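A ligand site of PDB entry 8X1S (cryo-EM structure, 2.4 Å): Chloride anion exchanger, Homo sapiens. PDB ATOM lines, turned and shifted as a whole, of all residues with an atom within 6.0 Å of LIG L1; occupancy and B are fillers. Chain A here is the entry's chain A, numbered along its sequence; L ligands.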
ATOM      1  N   SER A  93      21.153   2.966  10.112  1.00  0.00           N
ATOM      2  CA  SER A  93      21.681   1.655  10.416  1.00  0.00           C
ATOM      3  C   SER A  93      20.581   0.684  10.779  1.00  0.00           C
ATOM      4  O   SER A  93      20.516  -0.426  10.251  1.00  0.00           O
ATOM      5  CB  SER A  93      22.695   1.763  11.555  1.00  0.00           C
ATOM      6  OG  SER A  93      23.710   2.695  11.239  1.00  0.00           O
ATOM      7  N   ILE A  96      18.231  -0.353   7.784  1.00  0.00           N
ATOM      8  CA  ILE A  96      18.713  -1.431   6.934  1.00  0.00           C
ATOM      9  C   ILE A  96      18.486  -2.787   7.587  1.00  0.00           C
ATOM     10  O   ILE A  96      18.004  -3.715   6.944  1.00  0.00           O
ATOM     11  CB  ILE A  96      20.211  -1.261   6.638  1.00  0.00           C
ATOM     12  CG1 ILE A  96      20.454   0.059   5.908  1.00  0.00           C
ATOM     13  CG2 ILE A  96      20.726  -2.431   5.820  1.00  0.00           C
ATOM     14  CD1 ILE A  96      21.912   0.328   5.616  1.00  0.00           C
ATOM     15  N   VAL A  97      18.807  -2.902   8.865  1.00  0.00           N
ATOM     16  CA  VAL A  97      18.613  -4.151   9.577  1.00  0.00           C
ATOM     17  C   VAL A  97      17.151  -4.518   9.577  1.00  0.00           C
ATOM     18  O   VAL A  97      16.794  -5.675   9.406  1.00  0.00           O
ATOM     19  CB  VAL A  97      19.141  -4.074  11.018  1.00  0.00           C
ATOM     20  CG1 VAL A  97      18.902  -5.377  11.751  1.00  0.00           C
ATOM     21  CG2 VAL A  97      20.620  -3.719  11.026  1.00  0.00           C
ATOM     22  N   LEU A 100      16.063  -6.076   6.210  1.00  0.00           N
ATOM     23  CA  LEU A 100      16.522  -7.443   6.024  1.00  0.00           C
ATOM     24  C   LEU A 100      15.879  -8.393   7.005  1.00  0.00           C
ATOM     25  O   LEU A 100      15.493  -9.501   6.650  1.00  0.00           O
ATOM     26  CB  LEU A 100      18.039  -7.513   6.125  1.00  0.00           C
ATOM     27  CG  LEU A 100      18.795  -6.845   4.976  1.00  0.00           C
ATOM     28  CD1 LEU A 100      20.277  -6.714   5.286  1.00  0.00           C
ATOM     29  CD2 LEU A 100      18.569  -7.611   3.686  1.00  0.00           C
ATOM     30  N   GLN A 101      15.752  -7.967   8.253  1.00  0.00           N
ATOM     31  CA  GLN A 101      15.112  -8.795   9.255  1.00  0.00           C
ATOM     32  C   GLN A 101      13.625  -8.917   8.966  1.00  0.00           C
ATOM     33  O   GLN A 101      13.041  -9.960   9.231  1.00  0.00           O
ATOM     34  CB  GLN A 101      15.366  -8.250  10.655  1.00  0.00           C
ATOM     35  CG  GLN A 101      16.768  -8.467  11.172  1.00  0.00           C
ATOM     36  CD  GLN A 101      16.895  -8.120  12.645  1.00  0.00           C
ATOM     37  OE1 GLN A 101      15.971  -7.561  13.238  1.00  0.00           O
ATOM     38  NE2 GLN A 101      18.033  -8.442  13.229  1.00  0.00           N
ATOM     39  N   ALA A 104      13.406 -11.676   6.353  1.00  0.00           N
ATOM     40  CA  ALA A 104      13.679 -12.986   6.940  1.00  0.00           C
ATOM     41  C   ALA A 104      12.543 -13.460   7.844  1.00  0.00           C
ATOM     42  O   ALA A 104      12.140 -14.624   7.817  1.00  0.00           O
ATOM     43  CB  ALA A 104      14.993 -12.943   7.704  1.00  0.00           C
ATOM     44  N   PHE A 105      11.997 -12.560   8.656  1.00  0.00           N
ATOM     45  CA  PHE A 105      10.983 -12.995   9.591  1.00  0.00           C
ATOM     46  C   PHE A 105       9.649 -13.192   8.899  1.00  0.00           C
ATOM     47  O   PHE A 105       8.818 -13.980   9.374  1.00  0.00           O
ATOM     48  CB  PHE A 105      10.891 -12.011  10.748  1.00  0.00           C
ATOM     49  CG  PHE A 105      12.206 -11.764  11.453  1.00  0.00           C
ATOM     50  CD1 PHE A 105      13.253 -12.647  11.323  1.00  0.00           C
ATOM     51  CD2 PHE A 105      12.381 -10.647  12.244  1.00  0.00           C
ATOM     52  CE1 PHE A 105      14.453 -12.419  11.950  1.00  0.00           C
ATOM     53  CE2 PHE A 105      13.569 -10.430  12.882  1.00  0.00           C
ATOM     54  CZ  PHE A 105      14.608 -11.307  12.730  1.00  0.00           C
ATOM     55  N   LYS A 287      31.809 -11.540  13.324  1.00  0.00           N
ATOM     56  CA  LYS A 287      31.039 -11.067  14.481  1.00  0.00           C
ATOM     57  C   LYS A 287      31.848 -11.162  15.745  1.00  0.00           C
ATOM     58  O   LYS A 287      31.768 -10.289  16.596  1.00  0.00           O
ATOM     59  CB  LYS A 287      29.745 -11.855  14.652  1.00  0.00           C
ATOM     60  CG  LYS A 287      28.508 -11.092  14.236  1.00  0.00           C
ATOM     61  CD  LYS A 287      27.261 -11.966  14.275  1.00  0.00           C
ATOM     62  CE  LYS A 287      26.046 -11.178  14.742  1.00  0.00           C
ATOM     63  NZ  LYS A 287      24.771 -11.720  14.233  1.00  0.00           N
ATOM     64  N   PRO A 302      30.453  -4.072   9.445  1.00  0.00           N
ATOM     65  CA  PRO A 302      29.061  -4.503   9.270  1.00  0.00           C
ATOM     66  C   PRO A 302      29.031  -5.727   8.366  1.00  0.00           C
ATOM     67  O   PRO A 302      28.754  -5.618   7.187  1.00  0.00           O
ATOM     68  CB  PRO A 302      28.400  -3.308   8.580  1.00  0.00           C
ATOM     69  CG  PRO A 302      29.520  -2.448   8.086  1.00  0.00           C
ATOM     70  CD  PRO A 302      30.839  -3.044   8.477  1.00  0.00           C
ATOM     71  N   GLU A 304      26.988  -8.490   8.311  1.00  0.00           N
ATOM     72  CA  GLU A 304      25.707  -8.929   7.810  1.00  0.00           C
ATOM     73  C   GLU A 304      25.280  -8.134   6.595  1.00  0.00           C
ATOM     74  O   GLU A 304      24.725  -8.685   5.657  1.00  0.00           O
ATOM     75  CB  GLU A 304      24.634  -8.832   8.891  1.00  0.00           C
ATOM     76  CG  GLU A 304      24.951  -9.568  10.174  1.00  0.00           C
ATOM     77  CD  GLU A 304      25.823  -8.746  11.093  1.00  0.00           C
ATOM     78  OE1 GLU A 304      26.049  -9.168  12.234  1.00  0.00           O
ATOM     79  OE2 GLU A 304      26.279  -7.664  10.687  1.00  0.00           O
ATOM     80  N   PHE A 305      25.492  -6.832   6.625  1.00  0.00           N
ATOM     81  CA  PHE A 305      25.150  -6.004   5.485  1.00  0.00           C
ATOM     82  C   PHE A 305      26.043  -6.297   4.288  1.00  0.00           C
ATOM     83  O   PHE A 305      25.578  -6.399   3.170  1.00  0.00           O
ATOM     84  CB  PHE A 305      25.222  -4.519   5.845  1.00  0.00           C
ATOM     85  CG  PHE A 305      24.783  -3.618   4.746  1.00  0.00           C
ATOM     86  CD1 PHE A 305      23.477  -3.614   4.316  1.00  0.00           C
ATOM     87  CD2 PHE A 305      25.677  -2.768   4.132  1.00  0.00           C
ATOM     88  CE1 PHE A 305      23.056  -2.781   3.296  1.00  0.00           C
ATOM     89  CE2 PHE A 305      25.273  -1.933   3.114  1.00  0.00           C
ATOM     90  CZ  PHE A 305      23.958  -1.937   2.703  1.00  0.00           C
ATOM     91  N   THR A 308      24.977  -9.662   2.583  1.00  0.00           N
ATOM     92  CA  THR A 308      23.787  -9.604   1.752  1.00  0.00           C
ATOM     93  C   THR A 308      23.996  -8.907   0.436  1.00  0.00           C
ATOM     94  O   THR A 308      23.468  -9.324  -0.570  1.00  0.00           O
ATOM     95  CB  THR A 308      22.579  -8.954   2.450  1.00  0.00           C
ATOM     96  OG1 THR A 308      22.870  -7.578   2.685  1.00  0.00           O
ATOM     97  CG2 THR A 308      22.318  -9.617   3.743  1.00  0.00           C
ATOM     98  N   SER A 409      18.552  -7.839  18.984  1.00  0.00           N
ATOM     99  CA  SER A 409      19.673  -7.526  18.116  1.00  0.00           C
ATOM    100  C   SER A 409      19.521  -6.185  17.421  1.00  0.00           C
ATOM    101  O   SER A 409      20.482  -5.455  17.310  1.00  0.00           O
ATOM    102  CB  SER A 409      19.886  -8.636  17.092  1.00  0.00           C
ATOM    103  OG  SER A 409      18.859  -8.641  16.121  1.00  0.00           O
ATOM    104  N   ARG A 410      18.335  -5.882  16.928  1.00  0.00           N
ATOM    105  CA  ARG A 410      18.036  -4.606  16.274  1.00  0.00           C
ATOM    106  C   ARG A 410      18.090  -3.445  17.251  1.00  0.00           C
ATOM    107  O   ARG A 410      18.558  -2.369  16.925  1.00  0.00           O
ATOM    108  CB  ARG A 410      16.683  -4.672  15.551  1.00  0.00           C
ATOM    109  CG  ARG A 410      16.521  -3.722  14.377  1.00  0.00           C
ATOM    110  CD  ARG A 410      15.162  -3.862  13.698  1.00  0.00           C
ATOM    111  NE  ARG A 410      14.073  -3.948  14.660  1.00  0.00           N
ATOM    112  CZ  ARG A 410      13.312  -5.012  14.866  1.00  0.00           C
ATOM    113  NH1 ARG A 410      12.379  -4.984  15.774  1.00  0.00           N
ATOM    114  NH2 ARG A 410      13.486  -6.102  14.151  1.00  0.00           N
ATOM    115  N   VAL A 413      21.604  -2.563  17.988  1.00  0.00           N
ATOM    116  CA  VAL A 413      22.172  -1.782  16.910  1.00  0.00           C
ATOM    117  C   VAL A 413      21.759  -0.317  16.974  1.00  0.00           C
ATOM    118  O   VAL A 413      22.589   0.539  16.829  1.00  0.00           O
ATOM    119  CB  VAL A 413      21.759  -2.349  15.527  1.00  0.00           C
ATOM    120  CG1 VAL A 413      22.081  -1.359  14.428  1.00  0.00           C
ATOM    121  CG2 VAL A 413      22.442  -3.674  15.271  1.00  0.00           C
ATOM    122  N   LEU A 451      19.234 -15.220   3.840  1.00  0.00           N
ATOM    123  CA  LEU A 451      18.446 -14.558   4.882  1.00  0.00           C
ATOM    124  C   LEU A 451      18.333 -15.460   6.090  1.00  0.00           C
ATOM    125  O   LEU A 451      18.338 -14.993   7.219  1.00  0.00           O
ATOM    126  CB  LEU A 451      17.052 -14.214   4.381  1.00  0.00           C
ATOM    127  CG  LEU A 451      16.888 -13.008   3.473  1.00  0.00           C
ATOM    128  CD1 LEU A 451      15.463 -12.932   2.966  1.00  0.00           C
ATOM    129  CD2 LEU A 451      17.277 -11.724   4.184  1.00  0.00           C
ATOM    130  N   ALA A 452      18.131 -16.744   5.832  1.00  0.00           N
ATOM    131  CA  ALA A 452      18.042 -17.764   6.851  1.00  0.00           C
ATOM    132  C   ALA A 452      19.364 -17.901   7.601  1.00  0.00           C
ATOM    133  O   ALA A 452      19.369 -18.081   8.802  1.00  0.00           O
ATOM    134  CB  ALA A 452      17.623 -19.079   6.239  1.00  0.00           C
ATOM    135  N   LEU A 454      21.639 -15.567   8.095  1.00  0.00           N
ATOM    136  CA  LEU A 454      21.824 -14.404   8.946  1.00  0.00           C
ATOM    137  C   LEU A 454      21.093 -14.574  10.262  1.00  0.00           C
ATOM    138  O   LEU A 454      21.597 -14.222  11.318  1.00  0.00           O
ATOM    139  CB  LEU A 454      21.351 -13.148   8.256  1.00  0.00           C
ATOM    140  CG  LEU A 454      22.162 -12.749   7.033  1.00  0.00           C
ATOM    141  CD1 LEU A 454      21.441 -11.633   6.322  1.00  0.00           C
ATOM    142  CD2 LEU A 454      23.580 -12.356   7.400  1.00  0.00           C
ATOM    143  N   ALA A 455      19.883 -15.116  10.196  1.00  0.00           N
ATOM    144  CA  ALA A 455      19.067 -15.371  11.362  1.00  0.00           C
ATOM    145  C   ALA A 455      19.734 -16.395  12.277  1.00  0.00           C
ATOM    146  O   ALA A 455      19.657 -16.299  13.491  1.00  0.00           O
ATOM    147  CB  ALA A 455      17.678 -15.817  10.954  1.00  0.00           C
ATOM    148  N   ASN A 458      22.421 -14.991  14.657  1.00  0.00           N
ATOM    149  CA  ASN A 458      21.978 -14.338  15.898  1.00  0.00           C
ATOM    150  C   ASN A 458      21.594 -15.263  17.014  1.00  0.00           C
ATOM    151  O   ASN A 458      21.387 -14.837  18.134  1.00  0.00           O
ATOM    152  CB  ASN A 458      20.799 -13.448  15.627  1.00  0.00           C
ATOM    153  CG  ASN A 458      21.179 -12.271  14.828  1.00  0.00           C
ATOM    154  OD1 ASN A 458      22.244 -12.247  14.237  1.00  0.00           O
ATOM    155  ND2 ASN A 458      20.320 -11.280  14.808  1.00  0.00           N
HETATM  156  C1  LIG L   1      21.202  -8.707  11.547  1.00  0.00           C
HETATM  157  C2  LIG L   1      23.321  -5.799  10.994  1.00  0.00           C
HETATM  158  C3  LIG L   1      22.177  -6.106   8.943  1.00  0.00           C
HETATM  159  C4  LIG L   1      23.563  -6.999  13.788  1.00  0.00           C
HETATM  160  C5  LIG L   1      18.434 -10.722   8.243  1.00  0.00           C
HETATM  161  C6  LIG L   1      17.920 -11.709   8.997  1.00  0.00           C
HETATM  162  C7  LIG L   1      21.703  -7.662  10.729  1.00  0.00           C
HETATM  163  C8  LIG L   1      22.643  -6.908  11.487  1.00  0.00           C
HETATM  164  C9  LIG L   1      21.862  -8.542  12.732  1.00  0.00           C
HETATM  165  C10 LIG L   1      21.484  -7.214   9.419  1.00  0.00           C
HETATM  166  C11 LIG L   1      20.269  -9.816  11.382  1.00  0.00           C
HETATM  167  C12 LIG L   1      23.086  -5.392   9.697  1.00  0.00           C
HETATM  168  C13 LIG L   1      19.492 -10.275  10.233  1.00  0.00           C
HETATM  169  C14 LIG L   1      19.334  -9.893   8.943  1.00  0.00           C
HETATM  170  N1  LIG L   1      22.720  -7.453  12.717  1.00  0.00           N
HETATM  171  N2  LIG L   1      24.314  -5.944  13.578  1.00  0.00           N
HETATM  172  O1  LIG L   1      21.757  -9.272  13.855  1.00  0.00           O
HETATM  173  O2  LIG L   1      20.094 -10.510  12.371  1.00  0.00           O
HETATM  174  O3  LIG L   1      23.574  -7.570  14.859  1.00  0.00           O
HETATM  175  S1  LIG L   1      18.532 -11.671  10.603  1.00  0.00           S
HETATM  176 CL1  LIG L   1      21.959  -5.512   7.382  1.00  0.00          CL
HETATM  177  C1  LG2 L   2      26.269  -2.924  13.288  1.00  0.00           C
HETATM  178  O1  LG2 L   2      25.805  -1.767  12.598  1.00  0.00           O
HETATM  179  C2  LG2 L   2      26.857  -2.494  14.615  1.00  0.00           C
HETATM  180  O2  LG2 L   2      25.847  -1.886  15.421  1.00  0.00           O
HETATM  181  C3  LG2 L   2      27.431  -3.701  15.341  1.00  0.00           C
HETATM  182  C4  LG2 L   2      25.792  -1.949  11.190  1.00  0.00           C
HETATM  183  C5  LG2 L   2      24.389  -1.705  10.664  1.00  0.00           C
HETATM  184  O3  LG2 L   2      26.371  -4.419  15.962  1.00  0.00           O
HETATM  185  P1  LG2 L   2      26.594  -4.991  17.439  1.00  0.00           P
HETATM  186  O4  LG2 L   2      27.905  -4.444  17.940  1.00  0.00           O
HETATM  187  O5  LG2 L   2      25.329  -4.759  18.241  1.00  0.00           O
HETATM  188  O6  LG2 L   2      26.795  -6.574  17.232  1.00  0.00           O
HETATM  189  C6  LG2 L   2      26.318  -7.483  18.222  1.00  0.00           C
HETATM  190  C7  LG2 L   2      25.808  -8.758  17.567  1.00  0.00           C
HETATM  191  N1  LG2 L   2      24.903  -9.482  18.469  1.00  0.00           N
HETATM  192  C8  LG2 L   2      25.711 -10.390  19.278  1.00  0.00           C
HETATM  193  C9  LG2 L   2      24.184  -8.551  19.356  1.00  0.00           C
HETATM  194  C10 LG2 L   2      23.935 -10.262  17.688  1.00  0.00           C
HETATM  195  C11 LG2 L   2      24.388  -1.764   9.141  1.00  0.00           C
HETATM  196  C12 LG2 L   2      24.662  -0.382   8.549  1.00  0.00           C
HETATM  197  C13 LG2 L   2      25.559  -0.482   7.320  1.00  0.00           C
HETATM  198  C14 LG2 L   2      25.060   0.432   6.223  1.00  0.00           C
HETATM  199  C15 LG2 L   2      26.194   0.931   5.344  1.00  0.00           C
HETATM  200  C16 LG2 L   2      26.666   2.299   5.813  1.00  0.00           C
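ND2 of Asn 458 is in hydrogen-bond range of O2 of LIG L1, at 2.6 Å.
NE2 of Gln 101 sits at hydrogen-bond distance from O2 of LIG L1 (3.0 Å).
The backbone NH of Ala 455 lies close to a sulfur (S1) of LIG L1 (3.7 Å).
N2 of LIG L1 lies within hydrogen-bond range of O3 of LG2 L2 (3.5 Å).
OG of Ser 409 is in hydrogen-bond range of ND2 of Asn 458, at 3.3 Å.
The side-chain amide oxygen of Asn 458 is in hydrogen-bond range of the side-chain amino group of Lys 287 (2.6 Å).
The side-chain hydroxyl (OG) of Ser 409 lies within hydrogen-bond range of the side-chain amide nitrogen (NE2) of Gln 101 (3.0 Å).
OE1 of Gln 101 is in hydrogen-bond range of NH2 of Arg 410, at 3.0 Å.
The side-chain amino group (NZ) of Lys 287 lies within salt-bridge range of the side-chain carboxylate (OE1) of Glu 304 (3.5 Å).
The side-chain hydroxyl (OG1) of Thr 308 sits at hydrogen-bond distance from the backbone carbonyl oxygen (O) of Phe 305, 3.0 Å away.
Residues that only touch LIG L1: Ile 96, Val 97, Leu 100, Ala 104, Lys 287, Glu 304, Phe 305, Ser 409, Val 413, Leu 451 and Leu 454.
Hydrophobic or aromatic side chains within 4 Å of LIG L1: Ile 96, Val 97, Leu 100, Ala 104, Phe 305, Val 413 and Leu 454.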
